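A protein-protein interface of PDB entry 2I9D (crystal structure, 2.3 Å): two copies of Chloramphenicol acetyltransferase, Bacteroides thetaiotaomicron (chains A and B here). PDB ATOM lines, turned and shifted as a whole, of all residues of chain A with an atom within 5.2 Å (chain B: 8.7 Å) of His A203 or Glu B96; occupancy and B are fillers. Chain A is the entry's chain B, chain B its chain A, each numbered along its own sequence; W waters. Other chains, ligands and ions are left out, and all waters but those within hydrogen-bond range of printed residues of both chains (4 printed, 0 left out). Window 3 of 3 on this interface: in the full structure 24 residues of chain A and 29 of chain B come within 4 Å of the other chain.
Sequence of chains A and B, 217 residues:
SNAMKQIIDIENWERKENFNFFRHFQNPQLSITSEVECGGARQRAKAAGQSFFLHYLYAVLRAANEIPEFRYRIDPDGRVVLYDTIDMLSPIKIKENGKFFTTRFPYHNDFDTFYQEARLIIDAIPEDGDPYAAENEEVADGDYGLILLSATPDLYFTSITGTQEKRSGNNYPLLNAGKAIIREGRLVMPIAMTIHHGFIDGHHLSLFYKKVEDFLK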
ATOM      1  N   ASP A 201       5.984 -13.541 -11.586  1.00  0.00           N
ATOM      2  CA  ASP A 201       4.722 -14.290 -11.665  1.00  0.00           C
ATOM      3  C   ASP A 201       3.715 -13.740 -10.676  1.00  0.00           C
ATOM      4  O   ASP A 201       4.044 -12.881  -9.860  1.00  0.00           O
ATOM      5  CB  ASP A 201       4.953 -15.778 -11.396  1.00  0.00           C
ATOM      6  CG  ASP A 201       5.980 -16.373 -12.339  1.00  0.00           C
ATOM      7  OD1 ASP A 201       5.946 -15.998 -13.533  1.00  0.00           O
ATOM      8  OD2 ASP A 201       6.842 -17.170 -11.886  1.00  0.00           O
ATOM      9  N   GLY A 202       2.489 -14.247 -10.761  1.00  0.00           N
ATOM     10  CA  GLY A 202       1.413 -13.959  -9.772  1.00  0.00           C
ATOM     11  C   GLY A 202       1.885 -14.169  -8.351  1.00  0.00           C
ATOM     12  O   GLY A 202       1.647 -13.340  -7.483  1.00  0.00           O
ATOM     13  N   HIS A 203       2.597 -15.272  -8.105  1.00  0.00           N
ATOM     14  CA  HIS A 203       3.209 -15.491  -6.794  1.00  0.00           C
ATOM     15  C   HIS A 203       3.957 -14.237  -6.276  1.00  0.00           C
ATOM     16  O   HIS A 203       3.729 -13.792  -5.158  1.00  0.00           O
ATOM     17  CB  HIS A 203       4.170 -16.682  -6.840  1.00  0.00           C
ATOM     18  CG  HIS A 203       4.955 -16.854  -5.579  1.00  0.00           C
ATOM     19  ND1 HIS A 203       4.453 -17.514  -4.479  1.00  0.00           N
ATOM     20  CD2 HIS A 203       6.188 -16.412  -5.229  1.00  0.00           C
ATOM     21  CE1 HIS A 203       5.347 -17.474  -3.504  1.00  0.00           C
ATOM     22  NE2 HIS A 203       6.411 -16.820  -3.938  1.00  0.00           N
ATOM     23  N   HIS A 204       4.854 -13.686  -7.092  1.00  0.00           N
ATOM     24  CA  HIS A 204       5.667 -12.513  -6.699  1.00  0.00           C
ATOM     25  C   HIS A 204       4.852 -11.223  -6.587  1.00  0.00           C
ATOM     26  O   HIS A 204       5.166 -10.356  -5.790  1.00  0.00           O
ATOM     27  CB  HIS A 204       6.853 -12.346  -7.668  1.00  0.00           C
ATOM     28  CG  HIS A 204       7.613 -13.616  -7.897  1.00  0.00           C
ATOM     29  ND1 HIS A 204       7.403 -14.425  -8.997  1.00  0.00           N
ATOM     30  CD2 HIS A 204       8.541 -14.251  -7.135  1.00  0.00           C
ATOM     31  CE1 HIS A 204       8.178 -15.492  -8.914  1.00  0.00           C
ATOM     32  NE2 HIS A 204       8.882 -15.407  -7.798  1.00  0.00           N
ATOM     33  N   LEU A 205       3.809 -11.104  -7.395  1.00  0.00           N
ATOM     34  CA  LEU A 205       2.885  -9.959  -7.325  1.00  0.00           C
ATOM     35  C   LEU A 205       2.111  -9.985  -6.020  1.00  0.00           C
ATOM     36  O   LEU A 205       1.921  -8.964  -5.369  1.00  0.00           O
ATOM     37  CB  LEU A 205       1.933  -9.969  -8.538  1.00  0.00           C
ATOM     38  CG  LEU A 205       2.616  -9.704  -9.894  1.00  0.00           C
ATOM     39  CD1 LEU A 205       1.731 -10.089 -11.117  1.00  0.00           C
ATOM     40  CD2 LEU A 205       3.174  -8.280 -10.027  1.00  0.00           C
ATOM     41  N   SER A 206       1.673 -11.175  -5.636  1.00  0.00           N
ATOM     42  CA  SER A 206       0.943 -11.366  -4.401  1.00  0.00           C
ATOM     43  C   SER A 206       1.837 -10.955  -3.197  1.00  0.00           C
ATOM     44  O   SER A 206       1.415 -10.195  -2.310  1.00  0.00           O
ATOM     45  CB  SER A 206       0.441 -12.804  -4.339  1.00  0.00           C
ATOM     46  OG  SER A 206      -0.313 -13.020  -3.177  1.00  0.00           O
ATOM     47  N   LEU A 207       3.088 -11.397  -3.213  1.00  0.00           N
ATOM     48  CA  LEU A 207       4.067 -11.000  -2.214  1.00  0.00           C
ATOM     49  C   LEU A 207       4.355  -9.510  -2.227  1.00  0.00           C
ATOM     50  O   LEU A 207       4.464  -8.895  -1.176  1.00  0.00           O
ATOM     51  CB  LEU A 207       5.376 -11.766  -2.438  1.00  0.00           C
ATOM     52  CG  LEU A 207       6.479 -11.943  -1.387  1.00  0.00           C
ATOM     53  CD1 LEU A 207       6.003 -11.862   0.105  1.00  0.00           C
ATOM     54  CD2 LEU A 207       7.183 -13.302  -1.651  1.00  0.00           C
ATOM     55  N   LYS B  93       1.061 -24.699  -8.431  1.00  0.00           N
ATOM     56  CA  LYS B  93       2.191 -24.360  -7.573  1.00  0.00           C
ATOM     57  C   LYS B  93       2.748 -25.646  -6.952  1.00  0.00           C
ATOM     58  O   LYS B  93       1.997 -26.434  -6.382  1.00  0.00           O
ATOM     59  CB  LYS B  93       1.773 -23.363  -6.490  1.00  0.00           C
ATOM     60  CG  LYS B  93       2.923 -22.795  -5.635  1.00  0.00           C
ATOM     61  CD  LYS B  93       2.340 -22.227  -4.347  1.00  0.00           C
ATOM     62  CE  LYS B  93       3.212 -21.139  -3.734  1.00  0.00           C
ATOM     63  NZ  LYS B  93       2.792 -20.846  -2.342  1.00  0.00           N
ATOM     64  N   ILE B  94       4.056 -25.864  -7.116  1.00  0.00           N
ATOM     65  CA  ILE B  94       4.734 -27.074  -6.627  1.00  0.00           C
ATOM     66  C   ILE B  94       5.691 -26.796  -5.457  1.00  0.00           C
ATOM     67  O   ILE B  94       6.010 -27.709  -4.704  1.00  0.00           O
ATOM     68  CB  ILE B  94       5.480 -27.889  -7.762  1.00  0.00           C
ATOM     69  CG1 ILE B  94       6.604 -27.073  -8.409  1.00  0.00           C
ATOM     70  CG2 ILE B  94       4.492 -28.426  -8.794  1.00  0.00           C
ATOM     71  CD1 ILE B  94       7.210 -27.683  -9.682  1.00  0.00           C
ATOM     72  N   LYS B  95       6.142 -25.549  -5.309  1.00  0.00           N
ATOM     73  CA  LYS B  95       7.061 -25.173  -4.224  1.00  0.00           C
ATOM     74  C   LYS B  95       6.646 -23.867  -3.560  1.00  0.00           C
ATOM     75  O   LYS B  95       5.980 -23.024  -4.172  1.00  0.00           O
ATOM     76  CB  LYS B  95       8.507 -25.077  -4.740  1.00  0.00           C
ATOM     77  CG  LYS B  95       9.175 -26.442  -4.943  1.00  0.00           C
ATOM     78  CD  LYS B  95      10.583 -26.345  -5.500  1.00  0.00           C
ATOM     79  CE  LYS B  95      11.064 -27.740  -5.949  1.00  0.00           C
ATOM     80  NZ  LYS B  95      12.260 -27.698  -6.873  1.00  0.00           N
ATOM     81  N   GLU B  96       7.061 -23.694  -2.308  1.00  0.00           N
ATOM     82  CA  GLU B  96       6.666 -22.519  -1.526  1.00  0.00           C
ATOM     83  C   GLU B  96       7.274 -21.180  -1.983  1.00  0.00           C
ATOM     84  O   GLU B  96       6.811 -20.119  -1.552  1.00  0.00           O
ATOM     85  CB  GLU B  96       6.887 -22.761  -0.023  1.00  0.00           C
ATOM     86  CG  GLU B  96       5.859 -23.739   0.582  1.00  0.00           C
ATOM     87  CD  GLU B  96       4.437 -23.542   0.002  1.00  0.00           C
ATOM     88  OE1 GLU B  96       3.726 -22.611   0.473  1.00  0.00           O
ATOM     89  OE2 GLU B  96       4.038 -24.319  -0.922  1.00  0.00           O
ATOM     90  N   ASN B  97       8.284 -21.244  -2.854  1.00  0.00           N
ATOM     91  CA  ASN B  97       8.895 -20.057  -3.459  1.00  0.00           C
ATOM     92  C   ASN B  97       8.228 -19.653  -4.782  1.00  0.00           C
ATOM     93  O   ASN B  97       8.776 -18.821  -5.536  1.00  0.00           O
ATOM     94  CB  ASN B  97      10.361 -20.321  -3.739  1.00  0.00           C
ATOM     95  CG  ASN B  97      10.548 -21.311  -4.871  1.00  0.00           C
ATOM     96  OD1 ASN B  97       9.665 -22.141  -5.119  1.00  0.00           O
ATOM     97  ND2 ASN B  97      11.667 -21.209  -5.588  1.00  0.00           N
ATOM     98  N   GLY B  98       7.088 -20.278  -5.090  1.00  0.00           N
ATOM     99  CA  GLY B  98       6.318 -19.919  -6.270  1.00  0.00           C
ATOM    100  C   GLY B  98       6.428 -20.829  -7.473  1.00  0.00           C
ATOM    101  O   GLY B  98       5.602 -20.724  -8.397  1.00  0.00           O
ATOM    102  N   LYS B  99       7.427 -21.728  -7.475  1.00  0.00           N
ATOM    103  CA  LYS B  99       7.565 -22.703  -8.570  1.00  0.00           C
ATOM    104  C   LYS B  99       6.262 -23.413  -8.813  1.00  0.00           C
ATOM    105  O   LYS B  99       5.569 -23.829  -7.891  1.00  0.00           O
ATOM    106  CB  LYS B  99       8.694 -23.734  -8.356  1.00  0.00           C
ATOM    107  CG  LYS B  99       9.934 -23.400  -9.191  1.00  0.00           C
ATOM    108  CD  LYS B  99      10.892 -24.610  -9.397  1.00  0.00           C
ATOM    109  CE  LYS B  99      10.606 -25.414 -10.735  1.00  0.00           C
ATOM    110  NZ  LYS B  99      10.361 -24.529 -11.954  1.00  0.00           N
ATOM    111  N   PHE B 100       5.918 -23.513 -10.081  1.00  0.00           N
ATOM    112  CA  PHE B 100       4.696 -24.184 -10.466  1.00  0.00           C
ATOM    113  C   PHE B 100       5.032 -25.119 -11.608  1.00  0.00           C
ATOM    114  O   PHE B 100       6.066 -24.979 -12.256  1.00  0.00           O
ATOM    115  CB  PHE B 100       3.653 -23.153 -10.927  1.00  0.00           C
ATOM    116  CG  PHE B 100       4.127 -22.294 -12.060  1.00  0.00           C
ATOM    117  CD1 PHE B 100       3.972 -22.711 -13.379  1.00  0.00           C
ATOM    118  CD2 PHE B 100       4.745 -21.070 -11.810  1.00  0.00           C
ATOM    119  CE1 PHE B 100       4.399 -21.911 -14.428  1.00  0.00           C
ATOM    120  CE2 PHE B 100       5.197 -20.280 -12.865  1.00  0.00           C
ATOM    121  CZ  PHE B 100       5.022 -20.699 -14.171  1.00  0.00           C
ATOM    122  N   SER B 150      -4.660 -19.203 -14.238  1.00  0.00           N
ATOM    123  CA  SER B 150      -3.621 -19.099 -13.229  1.00  0.00           C
ATOM    124  C   SER B 150      -4.232 -18.552 -11.916  1.00  0.00           C
ATOM    125  O   SER B 150      -4.856 -17.503 -11.934  1.00  0.00           O
ATOM    126  CB  SER B 150      -2.498 -18.209 -13.767  1.00  0.00           C
ATOM    127  OG  SER B 150      -1.652 -17.842 -12.702  1.00  0.00           O
ATOM    128  N   ALA B 151      -4.082 -19.285 -10.801  1.00  0.00           N
ATOM    129  CA  ALA B 151      -4.650 -18.857  -9.509  1.00  0.00           C
ATOM    130  C   ALA B 151      -3.679 -18.054  -8.677  1.00  0.00           C
ATOM    131  O   ALA B 151      -2.512 -18.426  -8.566  1.00  0.00           O
ATOM    132  CB  ALA B 151      -5.149 -20.054  -8.693  1.00  0.00           C
ATOM    133  N   THR B 152      -4.156 -16.963  -8.072  1.00  0.00           N
ATOM    134  CA  THR B 152      -3.386 -16.293  -7.054  1.00  0.00           C
ATOM    135  C   THR B 152      -4.295 -16.138  -5.862  1.00  0.00           C
ATOM    136  O   THR B 152      -4.884 -15.057  -5.666  1.00  0.00           O
ATOM    137  CB  THR B 152      -2.725 -14.920  -7.512  1.00  0.00           C
ATOM    138  OG1 THR B 152      -3.735 -13.948  -7.757  1.00  0.00           O
ATOM    139  CG2 THR B 152      -1.993 -15.112  -8.762  1.00  0.00           C
ATOM    140  N   PRO B 153      -4.418 -17.221  -5.058  1.00  0.00           N
ATOM    141  CA  PRO B 153      -5.443 -17.307  -4.029  1.00  0.00           C
ATOM    142  C   PRO B 153      -5.249 -16.370  -2.865  1.00  0.00           C
ATOM    143  O   PRO B 153      -6.194 -16.184  -2.101  1.00  0.00           O
ATOM    144  CB  PRO B 153      -5.377 -18.777  -3.571  1.00  0.00           C
ATOM    145  CG  PRO B 153      -3.951 -19.185  -3.843  1.00  0.00           C
ATOM    146  CD  PRO B 153      -3.597 -18.453  -5.116  1.00  0.00           C
ATOM    147  N   ASP B 154      -4.053 -15.791  -2.740  1.00  0.00           N
ATOM    148  CA  ASP B 154      -3.720 -14.844  -1.666  1.00  0.00           C
ATOM    149  C   ASP B 154      -3.701 -13.368  -2.116  1.00  0.00           C
ATOM    150  O   ASP B 154      -3.263 -12.485  -1.354  1.00  0.00           O
ATOM    151  CB  ASP B 154      -2.357 -15.189  -1.037  1.00  0.00           C
ATOM    152  CG  ASP B 154      -2.336 -16.581  -0.401  1.00  0.00           C
ATOM    153  OD1 ASP B 154      -3.318 -16.958   0.278  1.00  0.00           O
ATOM    154  OD2 ASP B 154      -1.330 -17.297  -0.587  1.00  0.00           O
ATOM    155  N   LEU B 155      -4.164 -13.110  -3.344  1.00  0.00           N
ATOM    156  CA  LEU B 155      -4.201 -11.770  -3.895  1.00  0.00           C
ATOM    157  C   LEU B 155      -5.575 -11.415  -4.464  1.00  0.00           C
ATOM    158  O   LEU B 155      -6.091 -12.115  -5.340  1.00  0.00           O
ATOM    159  CB  LEU B 155      -3.148 -11.639  -5.004  1.00  0.00           C
ATOM    160  CG  LEU B 155      -3.006 -10.285  -5.727  1.00  0.00           C
ATOM    161  CD1 LEU B 155      -2.829  -9.132  -4.733  1.00  0.00           C
ATOM    162  CD2 LEU B 155      -1.865 -10.309  -6.758  1.00  0.00           C
ATOM    163  N   ASN B 176      -7.054 -15.447 -15.040  1.00  0.00           N
ATOM    164  CA  ASN B 176      -6.493 -15.317 -13.721  1.00  0.00           C
ATOM    165  C   ASN B 176      -7.612 -15.291 -12.718  1.00  0.00           C
ATOM    166  O   ASN B 176      -8.611 -14.571 -12.922  1.00  0.00           O
ATOM    167  CB  ASN B 176      -5.765 -13.995 -13.606  1.00  0.00           C
ATOM    168  CG  ASN B 176      -4.564 -13.919 -14.515  1.00  0.00           C
ATOM    169  OD1 ASN B 176      -3.477 -14.375 -14.156  1.00  0.00           O
ATOM    170  ND2 ASN B 176      -4.742 -13.315 -15.684  1.00  0.00           N
HETATM  171  O   HOH W   1      10.682 -16.834  -6.217  1.00  0.00           O
HETATM  172  O   HOH W   2      -1.334 -15.670  -4.240  1.00  0.00           O
HETATM  173  O   HOH W   3       9.206 -18.595  -8.497  1.00  0.00           O
HETATM  174  O   HOH W   4      -1.298 -10.314  -1.548  1.00  0.00           O
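The backbone carbonyl oxygen of Asn B97 sits close to a ring nitrogen (NE2) of His A203 (3.5 Å).
A ring nitrogen (ND1) of His A204 lies within hydrogen-bond range of the backbone NH (N) of Asp A201.
The side-chain amino group (NZ) of Lys B93 is in salt-bridge range of the side-chain carboxylate (OE1) of Glu B96, 3.5 Å away.
The backbone NH (N) of Lys B99 sits at hydrogen-bond distance from the side-chain amide oxygen (OD1) of Asn B97, at 3.3 Å.
Among the printed residues, pairs that only touch across the chains: Asp A201 with Phe B100 (3.7 Å), Gly A202 with Thr B152 (3.7 Å), His A203 with Lys B93 (3.9 Å), His A203 with Glu B96 (3.6 Å), His A203 with Gly B98 (3.4 Å), Ser A206 with Asp B154 (3.5 Å) and Ser A206 with Leu B155 (3.6 Å).
Glu B96 touches one residue of chain A.
Gly A202 touches just one residue of chain B: Thr B152 (3.7 Å).
His A204 touches none of the printed residues of chain B.
Of the printed residues of chain B, Asp A201 touches Phe B100 (3.7 Å).
Of the printed residues of chain B, Ser A206 touches Asp B154 (3.5 Å) and Leu B155 (3.6 Å).
Printed residues of chain A within 4 Å of Thr B152: Gly A202 (3.7 Å).
Of the printed residues of chain A, Asp B154 touches Ser A206 (3.5 Å).
Of the printed residues of chain A, Leu B155 touches Ser A206 (3.6 Å).
The nearest residue of chain B that does not touch His A203 is Thr B152 (4.6 Å).
The nearest printed residue of chain A that does not touch Glu B96 is Leu A207 (6.8 Å).
The nearest printed residue of chain A that does not touch Lys B93 is His A204 (8.3 Å).
Hydrophobic or aromatic side chains of chain B that line the printed part of chain A: Phe B100 and Leu B155.
Hydrophobic or aromatic side chains of chain A that line the printed part of chain B: His A203.
Along chain A the printed residues that touch a printed residue of chain B span positions 201 to 206.
Among the printed residues, no Asp or Glu carboxylate lies within 4 Å of a Lys or Arg side-chain nitrogen of the other chain.
No position is printed for both chains.
Of the 8 pairs that touch across the chains among the printed residues, none has its exchanged pair printed and touching as well.
Water W1 lies within hydrogen-bond range of a ring nitrogen (NE2) of His A204 and the backbone carbonyl oxygen (O) of Asn B97.
Water W4 lies within hydrogen-bond range of the backbone carbonyl oxygen (O) of Ser A206 (2.8 Å) and the backbone carbonyl oxygen (O) of Asp B154 (2.9 Å).
Water W3 lies within hydrogen-bond range of O of Asn B97 (3.0 Å) and NE2 of His A204 (3.3 Å).
Water W2 lies within hydrogen-bond range of the side-chain hydroxyl (OG) of Ser A206 (3.0 Å) and the backbone NH (N) of Asp B154 (3.1 Å).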
